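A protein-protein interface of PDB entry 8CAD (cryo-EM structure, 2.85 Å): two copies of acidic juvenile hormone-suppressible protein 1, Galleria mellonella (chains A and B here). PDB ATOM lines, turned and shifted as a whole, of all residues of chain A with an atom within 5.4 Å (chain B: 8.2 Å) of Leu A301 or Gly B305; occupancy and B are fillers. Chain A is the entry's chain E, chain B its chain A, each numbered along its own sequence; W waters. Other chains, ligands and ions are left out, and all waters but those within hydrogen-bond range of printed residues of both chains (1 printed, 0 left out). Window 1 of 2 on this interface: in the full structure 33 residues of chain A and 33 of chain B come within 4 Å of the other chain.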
ATOM      1  N   SER A 167     -18.292   1.753 -13.009  1.00  0.00           N
ATOM      2  CA  SER A 167     -19.205   1.563 -11.888  1.00  0.00           C
ATOM      3  C   SER A 167     -19.219   2.740 -10.922  1.00  0.00           C
ATOM      4  O   SER A 167     -20.132   2.822 -10.093  1.00  0.00           O
ATOM      5  CB  SER A 167     -18.833   0.287 -11.132  1.00  0.00           C
ATOM      6  OG  SER A 167     -17.516   0.370 -10.616  1.00  0.00           O
ATOM      7  N   HIS A 170     -22.028   5.591 -12.873  1.00  0.00           N
ATOM      8  CA  HIS A 170     -23.379   5.265 -13.306  1.00  0.00           C
ATOM      9  C   HIS A 170     -24.082   4.480 -12.209  1.00  0.00           C
ATOM     10  O   HIS A 170     -23.440   3.810 -11.396  1.00  0.00           O
ATOM     11  CB  HIS A 170     -23.370   4.460 -14.612  1.00  0.00           C
ATOM     12  CG  HIS A 170     -22.518   5.063 -15.686  1.00  0.00           C
ATOM     13  ND1 HIS A 170     -22.929   6.134 -16.449  1.00  0.00           N
ATOM     14  CD2 HIS A 170     -21.276   4.747 -16.121  1.00  0.00           C
ATOM     15  CE1 HIS A 170     -21.978   6.452 -17.308  1.00  0.00           C
ATOM     16  NE2 HIS A 170     -20.964   5.625 -17.131  1.00  0.00           N
ATOM     17  N   GLY A 172     -26.379   1.704 -10.202  1.00  0.00           N
ATOM     18  CA  GLY A 172     -26.317   0.252 -10.211  1.00  0.00           C
ATOM     19  C   GLY A 172     -27.331  -0.384 -11.140  1.00  0.00           C
ATOM     20  O   GLY A 172     -27.062  -1.432 -11.737  1.00  0.00           O
ATOM     21  N   GLU A 173     -28.510   0.226 -11.268  1.00  0.00           N
ATOM     22  CA  GLU A 173     -29.520  -0.308 -12.176  1.00  0.00           C
ATOM     23  C   GLU A 173     -29.008  -0.319 -13.610  1.00  0.00           C
ATOM     24  O   GLU A 173     -29.232  -1.285 -14.350  1.00  0.00           O
ATOM     25  CB  GLU A 173     -30.804   0.516 -12.068  1.00  0.00           C
ATOM     26  CG  GLU A 173     -31.961  -0.023 -12.891  1.00  0.00           C
ATOM     27  CD  GLU A 173     -33.252   0.735 -12.649  1.00  0.00           C
ATOM     28  OE1 GLU A 173     -33.247   1.671 -11.821  1.00  0.00           O
ATOM     29  OE2 GLU A 173     -34.271   0.395 -13.286  1.00  0.00           O
ATOM     30  N   THR A 176     -26.519  -3.251 -13.957  1.00  0.00           N
ATOM     31  CA  THR A 176     -27.203  -4.539 -13.978  1.00  0.00           C
ATOM     32  C   THR A 176     -27.915  -4.753 -15.308  1.00  0.00           C
ATOM     33  O   THR A 176     -27.867  -5.848 -15.885  1.00  0.00           O
ATOM     34  CB  THR A 176     -28.189  -4.626 -12.812  1.00  0.00           C
ATOM     35  OG1 THR A 176     -27.502  -4.364 -11.580  1.00  0.00           O
ATOM     36  CG2 THR A 176     -28.827  -6.005 -12.746  1.00  0.00           C
ATOM     37  N   GLY A 299     -27.058   5.855  -4.585  1.00  0.00           N
ATOM     38  CA  GLY A 299     -27.600   5.012  -5.626  1.00  0.00           C
ATOM     39  C   GLY A 299     -26.562   4.247  -6.412  1.00  0.00           C
ATOM     40  O   GLY A 299     -26.906   3.630  -7.427  1.00  0.00           O
ATOM     41  N   LEU A 300     -25.307   4.263  -5.975  1.00  0.00           N
ATOM     42  CA  LEU A 300     -24.214   3.584  -6.653  1.00  0.00           C
ATOM     43  C   LEU A 300     -23.937   2.239  -5.992  1.00  0.00           C
ATOM     44  O   LEU A 300     -24.287   2.002  -4.834  1.00  0.00           O
ATOM     45  CB  LEU A 300     -22.948   4.445  -6.630  1.00  0.00           C
ATOM     46  CG  LEU A 300     -23.011   5.774  -7.385  1.00  0.00           C
ATOM     47  CD1 LEU A 300     -21.833   6.656  -7.004  1.00  0.00           C
ATOM     48  CD2 LEU A 300     -23.035   5.538  -8.884  1.00  0.00           C
ATOM     49  N   LEU A 301     -23.301   1.351  -6.754  1.00  0.00           N
ATOM     50  CA  LEU A 301     -22.936   0.026  -6.280  1.00  0.00           C
ATOM     51  C   LEU A 301     -21.481  -0.256  -6.625  1.00  0.00           C
ATOM     52  O   LEU A 301     -20.994   0.122  -7.694  1.00  0.00           O
ATOM     53  CB  LEU A 301     -23.831  -1.061  -6.897  1.00  0.00           C
ATOM     54  CG  LEU A 301     -25.318  -1.029  -6.539  1.00  0.00           C
ATOM     55  CD1 LEU A 301     -26.081  -2.053  -7.363  1.00  0.00           C
ATOM     56  CD2 LEU A 301     -25.521  -1.281  -5.055  1.00  0.00           C
ATOM     57  N   TYR A 302     -20.791  -0.925  -5.705  1.00  0.00           N
ATOM     58  CA  TYR A 302     -19.422  -1.344  -5.959  1.00  0.00           C
ATOM     59  C   TYR A 302     -19.398  -2.503  -6.951  1.00  0.00           C
ATOM     60  O   TYR A 302     -20.428  -3.100  -7.277  1.00  0.00           O
ATOM     61  CB  TYR A 302     -18.731  -1.753  -4.657  1.00  0.00           C
ATOM     62  CG  TYR A 302     -18.353  -0.589  -3.770  1.00  0.00           C
ATOM     63  CD1 TYR A 302     -17.254   0.204  -4.065  1.00  0.00           C
ATOM     64  CD2 TYR A 302     -19.091  -0.289  -2.634  1.00  0.00           C
ATOM     65  CE1 TYR A 302     -16.903   1.268  -3.257  1.00  0.00           C
ATOM     66  CE2 TYR A 302     -18.747   0.772  -1.819  1.00  0.00           C
ATOM     67  CZ  TYR A 302     -17.653   1.547  -2.137  1.00  0.00           C
ATOM     68  OH  TYR A 302     -17.307   2.605  -1.328  1.00  0.00           O
ATOM     69  N   HIS A 303     -18.196  -2.812  -7.443  1.00  0.00           N
ATOM     70  CA  HIS A 303     -18.055  -3.875  -8.433  1.00  0.00           C
ATOM     71  C   HIS A 303     -18.628  -5.189  -7.916  1.00  0.00           C
ATOM     72  O   HIS A 303     -19.365  -5.881  -8.627  1.00  0.00           O
ATOM     73  CB  HIS A 303     -16.586  -4.046  -8.819  1.00  0.00           C
ATOM     74  CG  HIS A 303     -16.365  -5.051  -9.904  1.00  0.00           C
ATOM     75  ND1 HIS A 303     -16.676  -4.802 -11.224  1.00  0.00           N
ATOM     76  CD2 HIS A 303     -15.873  -6.312  -9.865  1.00  0.00           C
ATOM     77  CE1 HIS A 303     -16.382  -5.865 -11.951  1.00  0.00           C
ATOM     78  NE2 HIS A 303     -15.894  -6.795 -11.150  1.00  0.00           N
ATOM     79  N   GLY A 305     -20.855  -5.594  -5.540  1.00  0.00           N
ATOM     80  CA  GLY A 305     -22.287  -5.438  -5.371  1.00  0.00           C
ATOM     81  C   GLY A 305     -22.692  -4.976  -3.987  1.00  0.00           C
ATOM     82  O   GLY A 305     -23.829  -5.203  -3.561  1.00  0.00           O
ATOM     83  N   ILE A 306     -21.776  -4.330  -3.274  1.00  0.00           N
ATOM     84  CA  ILE A 306     -22.052  -3.825  -1.931  1.00  0.00           C
ATOM     85  C   ILE A 306     -22.592  -2.402  -2.041  1.00  0.00           C
ATOM     86  O   ILE A 306     -21.938  -1.541  -2.648  1.00  0.00           O
ATOM     87  CB  ILE A 306     -20.798  -3.881  -1.045  1.00  0.00           C
ATOM     88  CG1 ILE A 306     -20.349  -5.334  -0.875  1.00  0.00           C
ATOM     89  CG2 ILE A 306     -21.076  -3.234   0.307  1.00  0.00           C
ATOM     90  CD1 ILE A 306     -19.098  -5.510  -0.041  1.00  0.00           C
ATOM     91  N   PRO A 307     -23.766  -2.103  -1.487  1.00  0.00           N
ATOM     92  CA  PRO A 307     -24.281  -0.732  -1.553  1.00  0.00           C
ATOM     93  C   PRO A 307     -23.409   0.242  -0.775  1.00  0.00           C
ATOM     94  O   PRO A 307     -22.727  -0.113   0.188  1.00  0.00           O
ATOM     95  CB  PRO A 307     -25.678  -0.842  -0.930  1.00  0.00           C
ATOM     96  CG  PRO A 307     -26.036  -2.278  -1.036  1.00  0.00           C
ATOM     97  CD  PRO A 307     -24.753  -3.025  -0.899  1.00  0.00           C
ATOM     98  N   TYR A 308     -23.445   1.500  -1.217  1.00  0.00           N
ATOM     99  CA  TYR A 308     -22.688   2.558  -0.569  1.00  0.00           C
ATOM    100  C   TYR A 308     -23.345   2.969   0.748  1.00  0.00           C
ATOM    101  O   TYR A 308     -24.554   2.800   0.928  1.00  0.00           O
ATOM    102  CB  TYR A 308     -22.584   3.774  -1.482  1.00  0.00           C
ATOM    103  CG  TYR A 308     -21.440   3.724  -2.468  1.00  0.00           C
ATOM    104  CD1 TYR A 308     -21.434   2.810  -3.511  1.00  0.00           C
ATOM    105  CD2 TYR A 308     -20.372   4.604  -2.363  1.00  0.00           C
ATOM    106  CE1 TYR A 308     -20.391   2.765  -4.415  1.00  0.00           C
ATOM    107  CE2 TYR A 308     -19.326   4.568  -3.263  1.00  0.00           C
ATOM    108  CZ  TYR A 308     -19.341   3.647  -4.287  1.00  0.00           C
ATOM    109  OH  TYR A 308     -18.301   3.607  -5.187  1.00  0.00           O
ATOM    110  N   GLY B  93     -41.687  -4.986 -13.463  1.00  0.00           N
ATOM    111  CA  GLY B  93     -40.324  -4.782 -13.001  1.00  0.00           C
ATOM    112  C   GLY B  93     -40.202  -3.719 -11.932  1.00  0.00           C
ATOM    113  O   GLY B  93     -39.236  -2.946 -11.938  1.00  0.00           O
ATOM    114  N   GLY B 172     -26.813  -9.223  -2.088  1.00  0.00           N
ATOM    115  CA  GLY B 172     -26.591  -8.810  -3.464  1.00  0.00           C
ATOM    116  C   GLY B 172     -25.272  -9.295  -4.029  1.00  0.00           C
ATOM    117  O   GLY B 172     -25.175  -9.593  -5.225  1.00  0.00           O
ATOM    118  N   THR B 176     -24.775 -11.229  -7.610  1.00  0.00           N
ATOM    119  CA  THR B 176     -23.875 -10.733  -8.646  1.00  0.00           C
ATOM    120  C   THR B 176     -22.820 -11.778  -8.992  1.00  0.00           C
ATOM    121  O   THR B 176     -22.509 -11.999 -10.169  1.00  0.00           O
ATOM    122  CB  THR B 176     -23.220  -9.429  -8.188  1.00  0.00           C
ATOM    123  OG1 THR B 176     -24.236  -8.487  -7.815  1.00  0.00           O
ATOM    124  CG2 THR B 176     -22.369  -8.833  -9.298  1.00  0.00           C
ATOM    125  N   ARG B 180     -22.162 -13.613 -12.601  1.00  0.00           N
ATOM    126  CA  ARG B 180     -20.847 -13.625 -13.234  1.00  0.00           C
ATOM    127  C   ARG B 180     -20.384 -15.051 -13.519  1.00  0.00           C
ATOM    128  O   ARG B 180     -19.924 -15.357 -14.626  1.00  0.00           O
ATOM    129  CB  ARG B 180     -19.839 -12.882 -12.356  1.00  0.00           C
ATOM    130  CG  ARG B 180     -20.092 -11.390 -12.282  1.00  0.00           C
ATOM    131  CD  ARG B 180     -19.073 -10.680 -11.413  1.00  0.00           C
ATOM    132  NE  ARG B 180     -19.348  -9.251 -11.307  1.00  0.00           N
ATOM    133  CZ  ARG B 180     -18.693  -8.416 -10.512  1.00  0.00           C
ATOM    134  NH1 ARG B 180     -17.714  -8.833  -9.725  1.00  0.00           N
ATOM    135  NH2 ARG B 180     -19.031  -7.129 -10.506  1.00  0.00           N
ATOM    136  N   LEU B 300     -29.396  -6.240   1.072  1.00  0.00           N
ATOM    137  CA  LEU B 300     -30.129  -6.879  -0.008  1.00  0.00           C
ATOM    138  C   LEU B 300     -30.303  -5.913  -1.175  1.00  0.00           C
ATOM    139  O   LEU B 300     -30.221  -4.692  -1.021  1.00  0.00           O
ATOM    140  CB  LEU B 300     -31.501  -7.358   0.479  1.00  0.00           C
ATOM    141  CG  LEU B 300     -31.503  -8.448   1.553  1.00  0.00           C
ATOM    142  CD1 LEU B 300     -32.884  -8.580   2.170  1.00  0.00           C
ATOM    143  CD2 LEU B 300     -31.053  -9.774   0.969  1.00  0.00           C
ATOM    144  N   LEU B 301     -30.541  -6.482  -2.354  1.00  0.00           N
ATOM    145  CA  LEU B 301     -30.756  -5.714  -3.570  1.00  0.00           C
ATOM    146  C   LEU B 301     -31.993  -6.231  -4.289  1.00  0.00           C
ATOM    147  O   LEU B 301     -32.255  -7.436  -4.323  1.00  0.00           O
ATOM    148  CB  LEU B 301     -29.543  -5.795  -4.509  1.00  0.00           C
ATOM    149  CG  LEU B 301     -28.230  -5.185  -4.012  1.00  0.00           C
ATOM    150  CD1 LEU B 301     -27.101  -5.505  -4.979  1.00  0.00           C
ATOM    151  CD2 LEU B 301     -28.368  -3.683  -3.831  1.00  0.00           C
ATOM    152  N   TYR B 302     -32.754  -5.304  -4.865  1.00  0.00           N
ATOM    153  CA  TYR B 302     -33.907  -5.677  -5.668  1.00  0.00           C
ATOM    154  C   TYR B 302     -33.454  -6.264  -7.002  1.00  0.00           C
ATOM    155  O   TYR B 302     -32.281  -6.194  -7.379  1.00  0.00           O
ATOM    156  CB  TYR B 302     -34.815  -4.470  -5.906  1.00  0.00           C
ATOM    157  CG  TYR B 302     -35.621  -4.060  -4.696  1.00  0.00           C
ATOM    158  CD1 TYR B 302     -36.741  -4.783  -4.306  1.00  0.00           C
ATOM    159  CD2 TYR B 302     -35.270  -2.946  -3.947  1.00  0.00           C
ATOM    160  CE1 TYR B 302     -37.482  -4.413  -3.203  1.00  0.00           C
ATOM    161  CE2 TYR B 302     -36.006  -2.567  -2.843  1.00  0.00           C
ATOM    162  CZ  TYR B 302     -37.111  -3.304  -2.475  1.00  0.00           C
ATOM    163  OH  TYR B 302     -37.846  -2.930  -1.375  1.00  0.00           O
ATOM    164  N   HIS B 303     -34.409  -6.861  -7.719  1.00  0.00           N
ATOM    165  CA  HIS B 303     -34.086  -7.498  -8.991  1.00  0.00           C
ATOM    166  C   HIS B 303     -33.424  -6.513  -9.948  1.00  0.00           C
ATOM    167  O   HIS B 303     -32.411  -6.830 -10.582  1.00  0.00           O
ATOM    168  CB  HIS B 303     -35.348  -8.088  -9.621  1.00  0.00           C
ATOM    169  CG  HIS B 303     -35.088  -8.845 -10.885  1.00  0.00           C
ATOM    170  ND1 HIS B 303     -34.503 -10.094 -10.898  1.00  0.00           N
ATOM    171  CD2 HIS B 303     -35.323  -8.527 -12.180  1.00  0.00           C
ATOM    172  CE1 HIS B 303     -34.394 -10.513 -12.145  1.00  0.00           C
ATOM    173  NE2 HIS B 303     -34.883  -9.581 -12.943  1.00  0.00           N
ATOM    174  N   ASN B 304     -33.986  -5.308 -10.069  1.00  0.00           N
ATOM    175  CA  ASN B 304     -33.400  -4.318 -10.969  1.00  0.00           C
ATOM    176  C   ASN B 304     -32.029  -3.860 -10.486  1.00  0.00           C
ATOM    177  O   ASN B 304     -31.138  -3.615 -11.307  1.00  0.00           O
ATOM    178  CB  ASN B 304     -34.335  -3.119 -11.121  1.00  0.00           C
ATOM    179  CG  ASN B 304     -34.694  -2.482  -9.795  1.00  0.00           C
ATOM    180  OD1 ASN B 304     -34.079  -2.766  -8.767  1.00  0.00           O
ATOM    181  ND2 ASN B 304     -35.695  -1.612  -9.811  1.00  0.00           N
ATOM    182  N   GLY B 305     -31.841  -3.744  -9.173  1.00  0.00           N
ATOM    183  CA  GLY B 305     -30.556  -3.358  -8.621  1.00  0.00           C
ATOM    184  C   GLY B 305     -30.614  -2.124  -7.745  1.00  0.00           C
ATOM    185  O   GLY B 305     -29.602  -1.440  -7.561  1.00  0.00           O
ATOM    186  N   ILE B 306     -31.789  -1.825  -7.199  1.00  0.00           N
ATOM    187  CA  ILE B 306     -31.966  -0.668  -6.326  1.00  0.00           C
ATOM    188  C   ILE B 306     -31.698  -1.091  -4.884  1.00  0.00           C
ATOM    189  O   ILE B 306     -32.329  -2.041  -4.396  1.00  0.00           O
ATOM    190  CB  ILE B 306     -33.369  -0.062  -6.480  1.00  0.00           C
ATOM    191  CG1 ILE B 306     -33.560   0.445  -7.911  1.00  0.00           C
ATOM    192  CG2 ILE B 306     -33.574   1.063  -5.471  1.00  0.00           C
ATOM    193  CD1 ILE B 306     -34.925   1.038  -8.190  1.00  0.00           C
ATOM    194  N   PRO B 307     -30.784  -0.438  -4.169  1.00  0.00           N
ATOM    195  CA  PRO B 307     -30.541  -0.810  -2.772  1.00  0.00           C
ATOM    196  C   PRO B 307     -31.752  -0.540  -1.891  1.00  0.00           C
ATOM    197  O   PRO B 307     -32.576   0.336  -2.160  1.00  0.00           O
ATOM    198  CB  PRO B 307     -29.356   0.073  -2.365  1.00  0.00           C
ATOM    199  CG  PRO B 307     -28.714   0.471  -3.643  1.00  0.00           C
ATOM    200  CD  PRO B 307     -29.822   0.576  -4.635  1.00  0.00           C
ATOM    201  N   TYR B 308     -31.847  -1.322  -0.815  1.00  0.00           N
ATOM    202  CA  TYR B 308     -32.932  -1.176   0.140  1.00  0.00           C
ATOM    203  C   TYR B 308     -32.724   0.059   1.017  1.00  0.00           C
ATOM    204  O   TYR B 308     -31.591   0.508   1.211  1.00  0.00           O
ATOM    205  CB  TYR B 308     -33.030  -2.412   1.026  1.00  0.00           C
ATOM    206  CG  TYR B 308     -33.853  -3.539   0.445  1.00  0.00           C
ATOM    207  CD1 TYR B 308     -33.418  -4.241  -0.668  1.00  0.00           C
ATOM    208  CD2 TYR B 308     -35.060  -3.908   1.021  1.00  0.00           C
ATOM    209  CE1 TYR B 308     -34.168  -5.274  -1.198  1.00  0.00           C
ATOM    210  CE2 TYR B 308     -35.815  -4.939   0.499  1.00  0.00           C
ATOM    211  CZ  TYR B 308     -35.365  -5.618  -0.610  1.00  0.00           C
ATOM    212  OH  TYR B 308     -36.113  -6.646  -1.134  1.00  0.00           O
ATOM    213  N   HIS B 481     -33.049 -16.966 -10.663  1.00  0.00           N
ATOM    214  CA  HIS B 481     -32.700 -15.563 -10.848  1.00  0.00           C
ATOM    215  C   HIS B 481     -31.820 -15.354 -12.074  1.00  0.00           C
ATOM    216  O   HIS B 481     -31.908 -14.308 -12.727  1.00  0.00           O
ATOM    217  CB  HIS B 481     -31.988 -15.024  -9.604  1.00  0.00           C
ATOM    218  CG  HIS B 481     -31.622 -13.574  -9.701  1.00  0.00           C
ATOM    219  ND1 HIS B 481     -32.529 -12.558  -9.486  1.00  0.00           N
ATOM    220  CD2 HIS B 481     -30.447 -12.972  -9.998  1.00  0.00           C
ATOM    221  CE1 HIS B 481     -31.925 -11.392  -9.643  1.00  0.00           C
ATOM    222  NE2 HIS B 481     -30.662 -11.617  -9.953  1.00  0.00           N
HETATM  223  O   HOH W   1     -29.139   1.915  -8.204  1.00  0.00           O
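The backbone carbonyl oxygen (O) of Gly A172 is in hydrogen-bond range of the side-chain hydroxyl (OG1) of Thr A176 (3.0 Å).
The backbone NH of Ile B306 lies within hydrogen-bond range of the side-chain amide oxygen of Asn B304, 2.9 Å away.
The guanidinium group (NH1) of Arg B180 lies within hydrogen-bond range of a ring nitrogen (NE2) of His A303 (3.1 Å).
Water W1 lies within hydrogen-bond range of O of Gly A299 (2.9 Å), N of Gly A172 (3.4 Å) and O of Gly B305 (3.4 Å).
Of chain B, only Leu B301, Gly B305 and Pro B307 come within 4 Å of Leu A301.
Gly B305 touches just one residue of chain A: Leu A301 (3.6 Å).
Of the printed residues of chain B, Thr A176 touches Asn B304 (3.5 Å).
Of the printed residues of chain B, His A303 touches Arg B180 (2.3 Å).
Of the printed residues of chain A, Pro B307 touches Leu A301.
Of the printed residues of chain A, Leu B301 touches Leu A301, Gly A305 and Pro A307.
Of the printed residues of chain A, Asn B304 touches Glu A173 (3.8 Å) and Thr A176 (3.5 Å).
Gly A172 touches none of the printed residues of chain B.
Tyr A302 touches none of the printed residues of chain B.
The nearest residue of chain A that does not touch Gly B305 is Glu A173 (4.2 Å).
Hydrophobic or aromatic side chains of chain A within 4 Å of the printed part of chain B: Leu A301, His A303 and Pro A307.
Hydrophobic or aromatic side chains of chain B that line the printed part of chain A: Leu B301 and Pro B307.
Among the printed residues, 8 pairs touch across the chains.
Leu A301 touches its own counterpart, Leu B301.
Leu A301 touches Gly B305, and with the chains exchanged Gly A305 touches Leu B301.
Leu A301 touches Pro B307, and with the chains exchanged Pro A307 touches Leu B301.
10 positions are printed for both chains.
Of the 8 pairs that touch across the chains among the printed residues, 5 have their exchanged pair printed and touching as well.
Glu A173 touches Asn B304 (CA to O, 3.8 Å).
Thr A176 touches Asn B304 (CB to O, 3.5 Å).
Leu A301 touches Leu B301.
Leu A301 touches Gly B305 (CD1 to O, 3.6 Å).
Leu A301 touches Pro B307.
Gly A305 touches Leu B301.
CG of Pro A307 touches CD2 of Leu B301, at 3.9 Å.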
